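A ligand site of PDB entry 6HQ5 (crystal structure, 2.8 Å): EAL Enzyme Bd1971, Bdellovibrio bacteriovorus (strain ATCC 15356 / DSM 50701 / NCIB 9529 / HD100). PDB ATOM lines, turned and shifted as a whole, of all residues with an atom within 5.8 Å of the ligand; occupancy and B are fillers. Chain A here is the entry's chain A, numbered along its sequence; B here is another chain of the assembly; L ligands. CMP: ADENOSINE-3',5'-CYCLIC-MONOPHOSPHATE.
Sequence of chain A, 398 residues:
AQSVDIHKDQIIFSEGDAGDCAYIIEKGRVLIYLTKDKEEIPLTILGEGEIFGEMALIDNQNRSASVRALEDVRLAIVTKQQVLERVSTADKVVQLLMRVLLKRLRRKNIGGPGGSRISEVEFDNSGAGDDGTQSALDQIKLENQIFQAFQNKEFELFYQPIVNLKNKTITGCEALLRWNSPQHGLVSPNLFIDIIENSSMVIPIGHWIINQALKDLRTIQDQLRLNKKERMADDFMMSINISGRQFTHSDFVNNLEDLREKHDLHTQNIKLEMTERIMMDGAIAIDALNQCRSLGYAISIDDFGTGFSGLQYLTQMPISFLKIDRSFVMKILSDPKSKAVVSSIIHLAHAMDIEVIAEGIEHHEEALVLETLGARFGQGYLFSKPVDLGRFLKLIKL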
ATOM      1  N   PHE A  13      38.621   7.703  -6.380  1.00  0.00           N
ATOM      2  CA  PHE A  13      38.696   9.142  -6.650  1.00  0.00           C
ATOM      3  C   PHE A  13      37.727   9.929  -5.751  1.00  0.00           C
ATOM      4  O   PHE A  13      36.869   9.346  -5.099  1.00  0.00           O
ATOM      5  CB  PHE A  13      38.469   9.453  -8.131  1.00  0.00           C
ATOM      6  CG  PHE A  13      37.165   8.940  -8.679  1.00  0.00           C
ATOM      7  CD1 PHE A  13      35.972   9.607  -8.410  1.00  0.00           C
ATOM      8  CD2 PHE A  13      37.131   7.815  -9.494  1.00  0.00           C
ATOM      9  CE1 PHE A  13      34.773   9.131  -8.930  1.00  0.00           C
ATOM     10  CE2 PHE A  13      35.932   7.346 -10.021  1.00  0.00           C
ATOM     11  CZ  PHE A  13      34.758   8.007  -9.729  1.00  0.00           C
ATOM     12  N   ILE A  32      29.521   4.843  -2.852  1.00  0.00           N
ATOM     13  CA  ILE A  32      29.372   6.143  -3.505  1.00  0.00           C
ATOM     14  C   ILE A  32      28.845   7.130  -2.480  1.00  0.00           C
ATOM     15  O   ILE A  32      27.764   6.929  -1.916  1.00  0.00           O
ATOM     16  CB  ILE A  32      28.363   6.073  -4.676  1.00  0.00           C
ATOM     17  CG1 ILE A  32      28.702   4.907  -5.634  1.00  0.00           C
ATOM     18  CG2 ILE A  32      28.316   7.402  -5.414  1.00  0.00           C
ATOM     19  CD1 ILE A  32      30.165   4.766  -5.972  1.00  0.00           C
ATOM     20  N   LEU A  43      25.337   7.614  -0.785  1.00  0.00           N
ATOM     21  CA  LEU A  43      24.319   7.489  -1.839  1.00  0.00           C
ATOM     22  C   LEU A  43      23.941   6.029  -2.031  1.00  0.00           C
ATOM     23  O   LEU A  43      22.767   5.670  -1.958  1.00  0.00           O
ATOM     24  CB  LEU A  43      24.797   8.107  -3.145  1.00  0.00           C
ATOM     25  CG  LEU A  43      25.063   9.607  -3.135  1.00  0.00           C
ATOM     26  CD1 LEU A  43      25.360  10.094  -4.545  1.00  0.00           C
ATOM     27  CD2 LEU A  43      23.887  10.376  -2.543  1.00  0.00           C
ATOM     28  N   THR A  44      24.940   5.184  -2.276  1.00  0.00           N
ATOM     29  CA  THR A  44      24.711   3.738  -2.361  1.00  0.00           C
ATOM     30  C   THR A  44      25.995   2.914  -2.221  1.00  0.00           C
ATOM     31  O   THR A  44      27.099   3.457  -2.180  1.00  0.00           O
ATOM     32  CB  THR A  44      24.052   3.343  -3.693  1.00  0.00           C
ATOM     33  OG1 THR A  44      23.666   1.971  -3.638  1.00  0.00           O
ATOM     34  CG2 THR A  44      24.990   3.567  -4.875  1.00  0.00           C
ATOM     35  N   LEU A  46      27.966  -0.233  -4.239  1.00  0.00           N
ATOM     36  CA  LEU A  46      28.005  -0.938  -5.528  1.00  0.00           C
ATOM     37  C   LEU A  46      28.836  -2.214  -5.419  1.00  0.00           C
ATOM     38  O   LEU A  46      30.028  -2.167  -5.121  1.00  0.00           O
ATOM     39  CB  LEU A  46      28.607  -0.039  -6.610  1.00  0.00           C
ATOM     40  CG  LEU A  46      27.821   1.218  -6.993  1.00  0.00           C
ATOM     41  CD1 LEU A  46      28.562   1.990  -8.064  1.00  0.00           C
ATOM     42  CD2 LEU A  46      26.416   0.871  -7.464  1.00  0.00           C
ATOM     43  N   ILE A  51      28.918  -0.783 -12.610  1.00  0.00           N
ATOM     44  CA  ILE A  51      29.841   0.145 -13.251  1.00  0.00           C
ATOM     45  C   ILE A  51      29.777   1.509 -12.562  1.00  0.00           C
ATOM     46  O   ILE A  51      28.709   1.936 -12.093  1.00  0.00           O
ATOM     47  CB  ILE A  51      29.517   0.265 -14.766  1.00  0.00           C
ATOM     48  CG1 ILE A  51      30.679   0.893 -15.557  1.00  0.00           C
ATOM     49  CG2 ILE A  51      28.198   1.012 -15.009  1.00  0.00           C
ATOM     50  CD1 ILE A  51      30.614   2.392 -15.748  1.00  0.00           C
ATOM     51  N   PHE A  52      30.909   2.194 -12.468  1.00  0.00           N
ATOM     52  CA  PHE A  52      30.941   3.558 -11.940  1.00  0.00           C
ATOM     53  C   PHE A  52      32.031   4.409 -12.574  1.00  0.00           C
ATOM     54  O   PHE A  52      32.918   3.904 -13.252  1.00  0.00           O
ATOM     55  CB  PHE A  52      31.088   3.533 -10.412  1.00  0.00           C
ATOM     56  CG  PHE A  52      32.463   3.175  -9.932  1.00  0.00           C
ATOM     57  CD1 PHE A  52      33.431   4.155  -9.754  1.00  0.00           C
ATOM     58  CD2 PHE A  52      32.794   1.851  -9.632  1.00  0.00           C
ATOM     59  CE1 PHE A  52      34.698   3.829  -9.315  1.00  0.00           C
ATOM     60  CE2 PHE A  52      34.053   1.521  -9.183  1.00  0.00           C
ATOM     61  CZ  PHE A  52      35.007   2.512  -9.022  1.00  0.00           C
ATOM     62  N   GLY A  53      31.945   5.709 -12.344  1.00  0.00           N
ATOM     63  CA  GLY A  53      32.887   6.676 -12.912  1.00  0.00           C
ATOM     64  C   GLY A  53      32.577   7.055 -14.349  1.00  0.00           C
ATOM     65  O   GLY A  53      33.417   7.644 -15.024  1.00  0.00           O
ATOM     66  N   GLU A  54      31.365   6.728 -14.809  1.00  0.00           N
ATOM     67  CA  GLU A  54      30.992   6.934 -16.214  1.00  0.00           C
ATOM     68  C   GLU A  54      30.476   8.342 -16.515  1.00  0.00           C
ATOM     69  O   GLU A  54      30.695   8.862 -17.607  1.00  0.00           O
ATOM     70  CB  GLU A  54      29.969   5.875 -16.661  1.00  0.00           C
ATOM     71  CG  GLU A  54      28.497   6.178 -16.353  1.00  0.00           C
ATOM     72  CD  GLU A  54      28.150   6.101 -14.877  1.00  0.00           C
ATOM     73  OE1 GLU A  54      28.965   5.560 -14.088  1.00  0.00           O
ATOM     74  OE2 GLU A  54      27.061   6.573 -14.509  1.00  0.00           O
ATOM     75  N   MET A  55      29.785   8.952 -15.553  1.00  0.00           N
ATOM     76  CA  MET A  55      29.122  10.233 -15.788  1.00  0.00           C
ATOM     77  C   MET A  55      30.088  11.320 -16.267  1.00  0.00           C
ATOM     78  O   MET A  55      29.838  11.990 -17.276  1.00  0.00           O
ATOM     79  CB  MET A  55      28.413  10.716 -14.519  1.00  0.00           C
ATOM     80  CG  MET A  55      27.221   9.862 -14.114  1.00  0.00           C
ATOM     81  SD  MET A  55      26.534  10.281 -12.498  1.00  0.00           S
ATOM     82  CE  MET A  55      25.831  11.893 -12.830  1.00  0.00           C
ATOM     83  N   ALA A  56      31.187  11.488 -15.538  1.00  0.00           N
ATOM     84  CA  ALA A  56      32.168  12.533 -15.823  1.00  0.00           C
ATOM     85  C   ALA A  56      32.677  12.491 -17.265  1.00  0.00           C
ATOM     86  O   ALA A  56      32.906  13.538 -17.875  1.00  0.00           O
ATOM     87  CB  ALA A  56      33.342  12.412 -14.861  1.00  0.00           C
ATOM     88  N   LEU A  57      32.838  11.289 -17.803  1.00  0.00           N
ATOM     89  CA  LEU A  57      33.430  11.104 -19.131  1.00  0.00           C
ATOM     90  C   LEU A  57      32.510  11.590 -20.252  1.00  0.00           C
ATOM     91  O   LEU A  57      32.973  12.255 -21.179  1.00  0.00           O
ATOM     92  CB  LEU A  57      33.748   9.629 -19.357  1.00  0.00           C
ATOM     93  CG  LEU A  57      34.659   8.927 -18.342  1.00  0.00           C
ATOM     94  CD1 LEU A  57      34.783   7.454 -18.688  1.00  0.00           C
ATOM     95  CD2 LEU A  57      36.027   9.577 -18.282  1.00  0.00           C
ATOM     96  N   ASN A  62      33.188  17.284 -13.957  1.00  0.00           N
ATOM     97  CA  ASN A  62      33.938  16.702 -12.856  1.00  0.00           C
ATOM     98  C   ASN A  62      33.240  15.510 -12.204  1.00  0.00           C
ATOM     99  O   ASN A  62      32.118  15.151 -12.579  1.00  0.00           O
ATOM    100  CB  ASN A  62      34.229  17.773 -11.798  1.00  0.00           C
ATOM    101  CG  ASN A  62      34.969  18.972 -12.350  1.00  0.00           C
ATOM    102  OD1 ASN A  62      35.555  18.920 -13.442  1.00  0.00           O
ATOM    103  ND2 ASN A  62      34.951  20.063 -11.604  1.00  0.00           N
ATOM    104  N   ARG A  63      33.908  14.898 -11.228  1.00  0.00           N
ATOM    105  CA  ARG A  63      33.352  13.760 -10.499  1.00  0.00           C
ATOM    106  C   ARG A  63      32.203  14.229  -9.613  1.00  0.00           C
ATOM    107  O   ARG A  63      32.394  15.078  -8.742  1.00  0.00           O
ATOM    108  CB  ARG A  63      34.436  13.084  -9.646  1.00  0.00           C
ATOM    109  CG  ARG A  63      35.586  12.472 -10.422  1.00  0.00           C
ATOM    110  CD  ARG A  63      35.132  11.417 -11.421  1.00  0.00           C
ATOM    111  NE  ARG A  63      36.226  10.544 -11.861  1.00  0.00           N
ATOM    112  CZ  ARG A  63      36.115   9.566 -12.752  1.00  0.00           C
ATOM    113  NH1 ARG A  63      34.948   9.297 -13.327  1.00  0.00           N
ATOM    114  NH2 ARG A  63      37.175   8.842 -13.073  1.00  0.00           N
ATOM    115  N   SER A  64      31.027  13.657  -9.836  1.00  0.00           N
ATOM    116  CA  SER A  64      29.819  14.040  -9.105  1.00  0.00           C
ATOM    117  C   SER A  64      29.733  13.444  -7.692  1.00  0.00           C
ATOM    118  O   SER A  64      28.806  13.777  -6.952  1.00  0.00           O
ATOM    119  CB  SER A  64      28.582  13.628  -9.898  1.00  0.00           C
ATOM    120  OG  SER A  64      28.448  12.208  -9.938  1.00  0.00           O
ATOM    121  N   ALA A  65      30.655  12.551  -7.336  1.00  0.00           N
ATOM    122  CA  ALA A  65      30.666  11.942  -6.010  1.00  0.00           C
ATOM    123  C   ALA A  65      32.010  11.292  -5.735  1.00  0.00           C
ATOM    124  O   ALA A  65      32.795  11.070  -6.653  1.00  0.00           O
ATOM    125  CB  ALA A  65      29.558  10.912  -5.889  1.00  0.00           C
ATOM    126  N   SER A  66      32.271  10.982  -4.461  1.00  0.00           N
ATOM    127  CA  SER A  66      33.489  10.259  -4.090  1.00  0.00           C
ATOM    128  C   SER A  66      33.215   8.763  -4.097  1.00  0.00           C
ATOM    129  O   SER A  66      32.071   8.325  -4.021  1.00  0.00           O
ATOM    130  CB  SER A  66      33.972  10.705  -2.706  1.00  0.00           C
ATOM    131  OG  SER A  66      34.415  12.049  -2.731  1.00  0.00           O
ATOM    132  N   VAL A  67      34.281   7.970  -4.194  1.00  0.00           N
ATOM    133  CA  VAL A  67      34.187   6.521  -4.220  1.00  0.00           C
ATOM    134  C   VAL A  67      35.288   5.928  -3.348  1.00  0.00           C
ATOM    135  O   VAL A  67      36.447   6.307  -3.474  1.00  0.00           O
ATOM    136  CB  VAL A  67      34.336   5.955  -5.651  1.00  0.00           C
ATOM    137  CG1 VAL A  67      33.968   4.485  -5.689  1.00  0.00           C
ATOM    138  CG2 VAL A  67      33.473   6.745  -6.627  1.00  0.00           C
ATOM    139  N   LEU A 105      20.510  13.638 -12.802  1.00  0.00           N
ATOM    140  CA  LEU A 105      21.147  12.849 -11.738  1.00  0.00           C
ATOM    141  C   LEU A 105      22.147  13.687 -10.940  1.00  0.00           C
ATOM    142  O   LEU A 105      22.315  13.478  -9.735  1.00  0.00           O
ATOM    143  CB  LEU A 105      21.820  11.594 -12.311  1.00  0.00           C
ATOM    144  CG  LEU A 105      22.254  10.517 -11.316  1.00  0.00           C
ATOM    145  CD1 LEU A 105      21.172  10.186 -10.315  1.00  0.00           C
ATOM    146  CD2 LEU A 105      22.692   9.264 -12.055  1.00  0.00           C
ATOM    147  N   ARG A 106      22.801  14.645 -11.597  1.00  0.00           N
ATOM    148  CA  ARG A 106      23.673  15.589 -10.907  1.00  0.00           C
ATOM    149  C   ARG A 106      22.889  16.645 -10.169  1.00  0.00           C
ATOM    150  O   ARG A 106      23.015  16.799  -8.951  1.00  0.00           O
ATOM    151  CB  ARG A 106      24.593  16.297 -11.897  1.00  0.00           C
ATOM    152  CG  ARG A 106      25.755  15.444 -12.329  1.00  0.00           C
ATOM    153  CD  ARG A 106      26.765  16.331 -13.028  1.00  0.00           C
ATOM    154  NE  ARG A 106      27.745  15.535 -13.743  1.00  0.00           N
ATOM    155  CZ  ARG A 106      27.610  15.113 -14.990  1.00  0.00           C
ATOM    156  NH1 ARG A 106      26.517  15.418 -15.687  1.00  0.00           N
ATOM    157  NH2 ARG A 106      28.564  14.388 -15.552  1.00  0.00           N
ATOM    158  N   LYS A 108      20.025  16.857  -9.122  1.00  0.00           N
ATOM    159  CA  LYS A 108      19.189  16.345  -8.048  1.00  0.00           C
ATOM    160  C   LYS A 108      19.982  15.794  -6.868  1.00  0.00           C
ATOM    161  O   LYS A 108      19.609  16.055  -5.719  1.00  0.00           O
ATOM    162  CB  LYS A 108      18.253  15.268  -8.603  1.00  0.00           C
ATOM    163  CG  LYS A 108      17.209  14.734  -7.631  1.00  0.00           C
ATOM    164  CD  LYS A 108      17.681  13.536  -6.830  1.00  0.00           C
ATOM    165  CE  LYS A 108      18.142  12.401  -7.737  1.00  0.00           C
ATOM    166  NZ  LYS A 108      17.854  11.051  -7.194  1.00  0.00           N
ATOM    167  N   ASN A 109      21.042  15.040  -7.131  1.00  0.00           N
ATOM    168  CA  ASN A 109      21.825  14.469  -6.017  1.00  0.00           C
ATOM    169  C   ASN A 109      22.498  15.563  -5.165  1.00  0.00           C
ATOM    170  O   ASN A 109      22.817  15.314  -4.002  1.00  0.00           O
ATOM    171  CB  ASN A 109      22.781  13.322  -6.464  1.00  0.00           C
ATOM    172  CG  ASN A 109      24.076  13.827  -7.060  1.00  0.00           C
ATOM    173  OD1 ASN A 109      24.145  14.897  -7.635  1.00  0.00           O
ATOM    174  ND2 ASN A 109      25.127  13.013  -6.943  1.00  0.00           N
ATOM    175  N   ARG B 104      19.122   4.497 -11.256  1.00  0.00           N
ATOM    176  CA  ARG B 104      19.688   5.368 -10.234  1.00  0.00           C
ATOM    177  C   ARG B 104      18.843   6.615 -10.003  1.00  0.00           C
ATOM    178  O   ARG B 104      18.704   7.061  -8.869  1.00  0.00           O
ATOM    179  CB  ARG B 104      21.126   5.748 -10.578  1.00  0.00           C
ATOM    180  CG  ARG B 104      22.097   4.602 -10.352  1.00  0.00           C
ATOM    181  CD  ARG B 104      23.444   4.816 -11.030  1.00  0.00           C
ATOM    182  NE  ARG B 104      24.311   3.648 -10.815  1.00  0.00           N
ATOM    183  CZ  ARG B 104      25.553   3.533 -11.277  1.00  0.00           C
ATOM    184  NH1 ARG B 104      26.096   4.510 -12.006  1.00  0.00           N
ATOM    185  NH2 ARG B 104      26.253   2.427 -11.027  1.00  0.00           N
ATOM    186  N   LYS B 108      16.967   6.503  -6.340  1.00  0.00           N
ATOM    187  CA  LYS B 108      17.385   7.585  -5.460  1.00  0.00           C
ATOM    188  C   LYS B 108      16.280   8.627  -5.207  1.00  0.00           C
ATOM    189  O   LYS B 108      16.146   9.101  -4.087  1.00  0.00           O
ATOM    190  CB  LYS B 108      18.695   8.222  -5.939  1.00  0.00           C
ATOM    191  CG  LYS B 108      19.851   7.237  -6.173  1.00  0.00           C
ATOM    192  CD  LYS B 108      19.902   6.060  -5.193  1.00  0.00           C
ATOM    193  CE  LYS B 108      21.182   5.257  -5.313  1.00  0.00           C
ATOM    194  NZ  LYS B 108      21.223   4.454  -6.561  1.00  0.00           N
HETATM  195  P   CMP L   1      31.234  10.216 -11.930  1.00  0.00           P
HETATM  196  O1P CMP L   1      32.203  10.256 -13.032  1.00  0.00           O
HETATM  197  O2P CMP L   1      30.439  11.430 -11.659  1.00  0.00           O
HETATM  198  O5' CMP L   1      32.021   9.811 -10.557  1.00  0.00           O
HETATM  199  C5' CMP L   1      31.176   9.560  -9.433  1.00  0.00           C
HETATM  200  C4' CMP L   1      30.398   8.328  -9.873  1.00  0.00           C
HETATM  201  O4' CMP L   1      29.503   7.830  -8.844  1.00  0.00           O
HETATM  202  C3' CMP L   1      29.481   8.745 -10.981  1.00  0.00           C
HETATM  203  O3' CMP L   1      30.256   8.923 -12.157  1.00  0.00           O
HETATM  204  C2' CMP L   1      28.549   7.572 -11.029  1.00  0.00           C
HETATM  205  O2' CMP L   1      29.163   6.481 -11.704  1.00  0.00           O
HETATM  206  C1' CMP L   1      28.360   7.234  -9.541  1.00  0.00           C
HETATM  207  N9  CMP L   1      27.093   7.825  -9.014  1.00  0.00           N
HETATM  208  C8  CMP L   1      26.811   9.127  -8.994  1.00  0.00           C
HETATM  209  N7  CMP L   1      25.603   9.283  -8.456  1.00  0.00           N
HETATM  210  C5  CMP L   1      25.132   8.080  -8.141  1.00  0.00           C
HETATM  211  C6  CMP L   1      23.975   7.712  -7.585  1.00  0.00           C
HETATM  212  N6  CMP L   1      23.123   8.676  -7.279  1.00  0.00           N
HETATM  213  N1  CMP L   1      23.684   6.427  -7.343  1.00  0.00           N
HETATM  214  C2  CMP L   1      24.638   5.456  -7.700  1.00  0.00           C
HETATM  215  N3  CMP L   1      25.841   5.882  -8.280  1.00  0.00           N
HETATM  216  C4  CMP L   1      26.061   7.185  -8.489  1.00  0.00           C
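O2P of the ligand sits at hydrogen-bond distance from N of Ser 64 (2.9 Å). NZ of Lys 108 of chain B lies within hydrogen-bond range of N1 of the ligand (3.2 Å). OG of Ser 64 lies within hydrogen-bond range of O2P of the ligand (2.7 Å). O2' of the ligand sits at hydrogen-bond distance from N of Gly 53 (3.0 Å). The side-chain carboxylate of Glu 54 lies within hydrogen-bond range of an oxygen (O2') of the ligand (2.6 Å). O1P of the ligand lies within salt-bridge range of NH1 of Arg 63, at 2.9 Å. O3' of the ligand sits at hydrogen-bond distance from N of Met 55 (3.4 Å). The backbone NH (N) of Ala 56 is in hydrogen-bond range of an oxygen (O1P) of the ligand, at 3.0 Å.
The backbone carbonyl oxygen of Met 55 sits at hydrogen-bond distance from the guanidinium group of Arg 106. The side-chain sulfur (SD) of Met 55 sits at hydrogen-bond distance from the side-chain hydroxyl (OG) of Ser 64. The guanidinium group of Arg 104 of chain B sits at hydrogen-bond distance from the backbone carbonyl oxygen of Ile 51 (2.7 Å). The backbone carbonyl oxygen (O) of Ile 32 sits at hydrogen-bond distance from the backbone NH (N) of Leu 43. The backbone carbonyl oxygen (O) of Leu 105 sits close to the side-chain amide oxygen (OD1) of Asn 109 (3.1 Å). The backbone carbonyl oxygen of Phe 13 sits at hydrogen-bond distance from the backbone NH of Val 67. The side-chain carboxylate of Glu 54 lies within salt-bridge range of the guanidinium group of Arg 104 of chain B (3.4 Å). The guanidinium group (NH1) of Arg 63 lies within hydrogen-bond range of the backbone carbonyl oxygen (O) of Gly 53 (2.8 Å).
Phe 13 touches the ligand (CE1 to O5', 3.3 Å). CG2 of Ile 32 touches O4' of the ligand (3.7 Å). Leu 43 touches the ligand. Thr 44 touches the ligand. CA of Phe 52 touches O2' of the ligand, at 3.4 Å. Ala 65 touches the ligand (O to C5', 3.6 Å). Leu 105 touches the ligand. CD of Arg 104 of chain B touches C2 of the ligand, 3.6 Å away. The nearest printed residue that does not touch the ligand is Asn 109 (4.1 Å).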
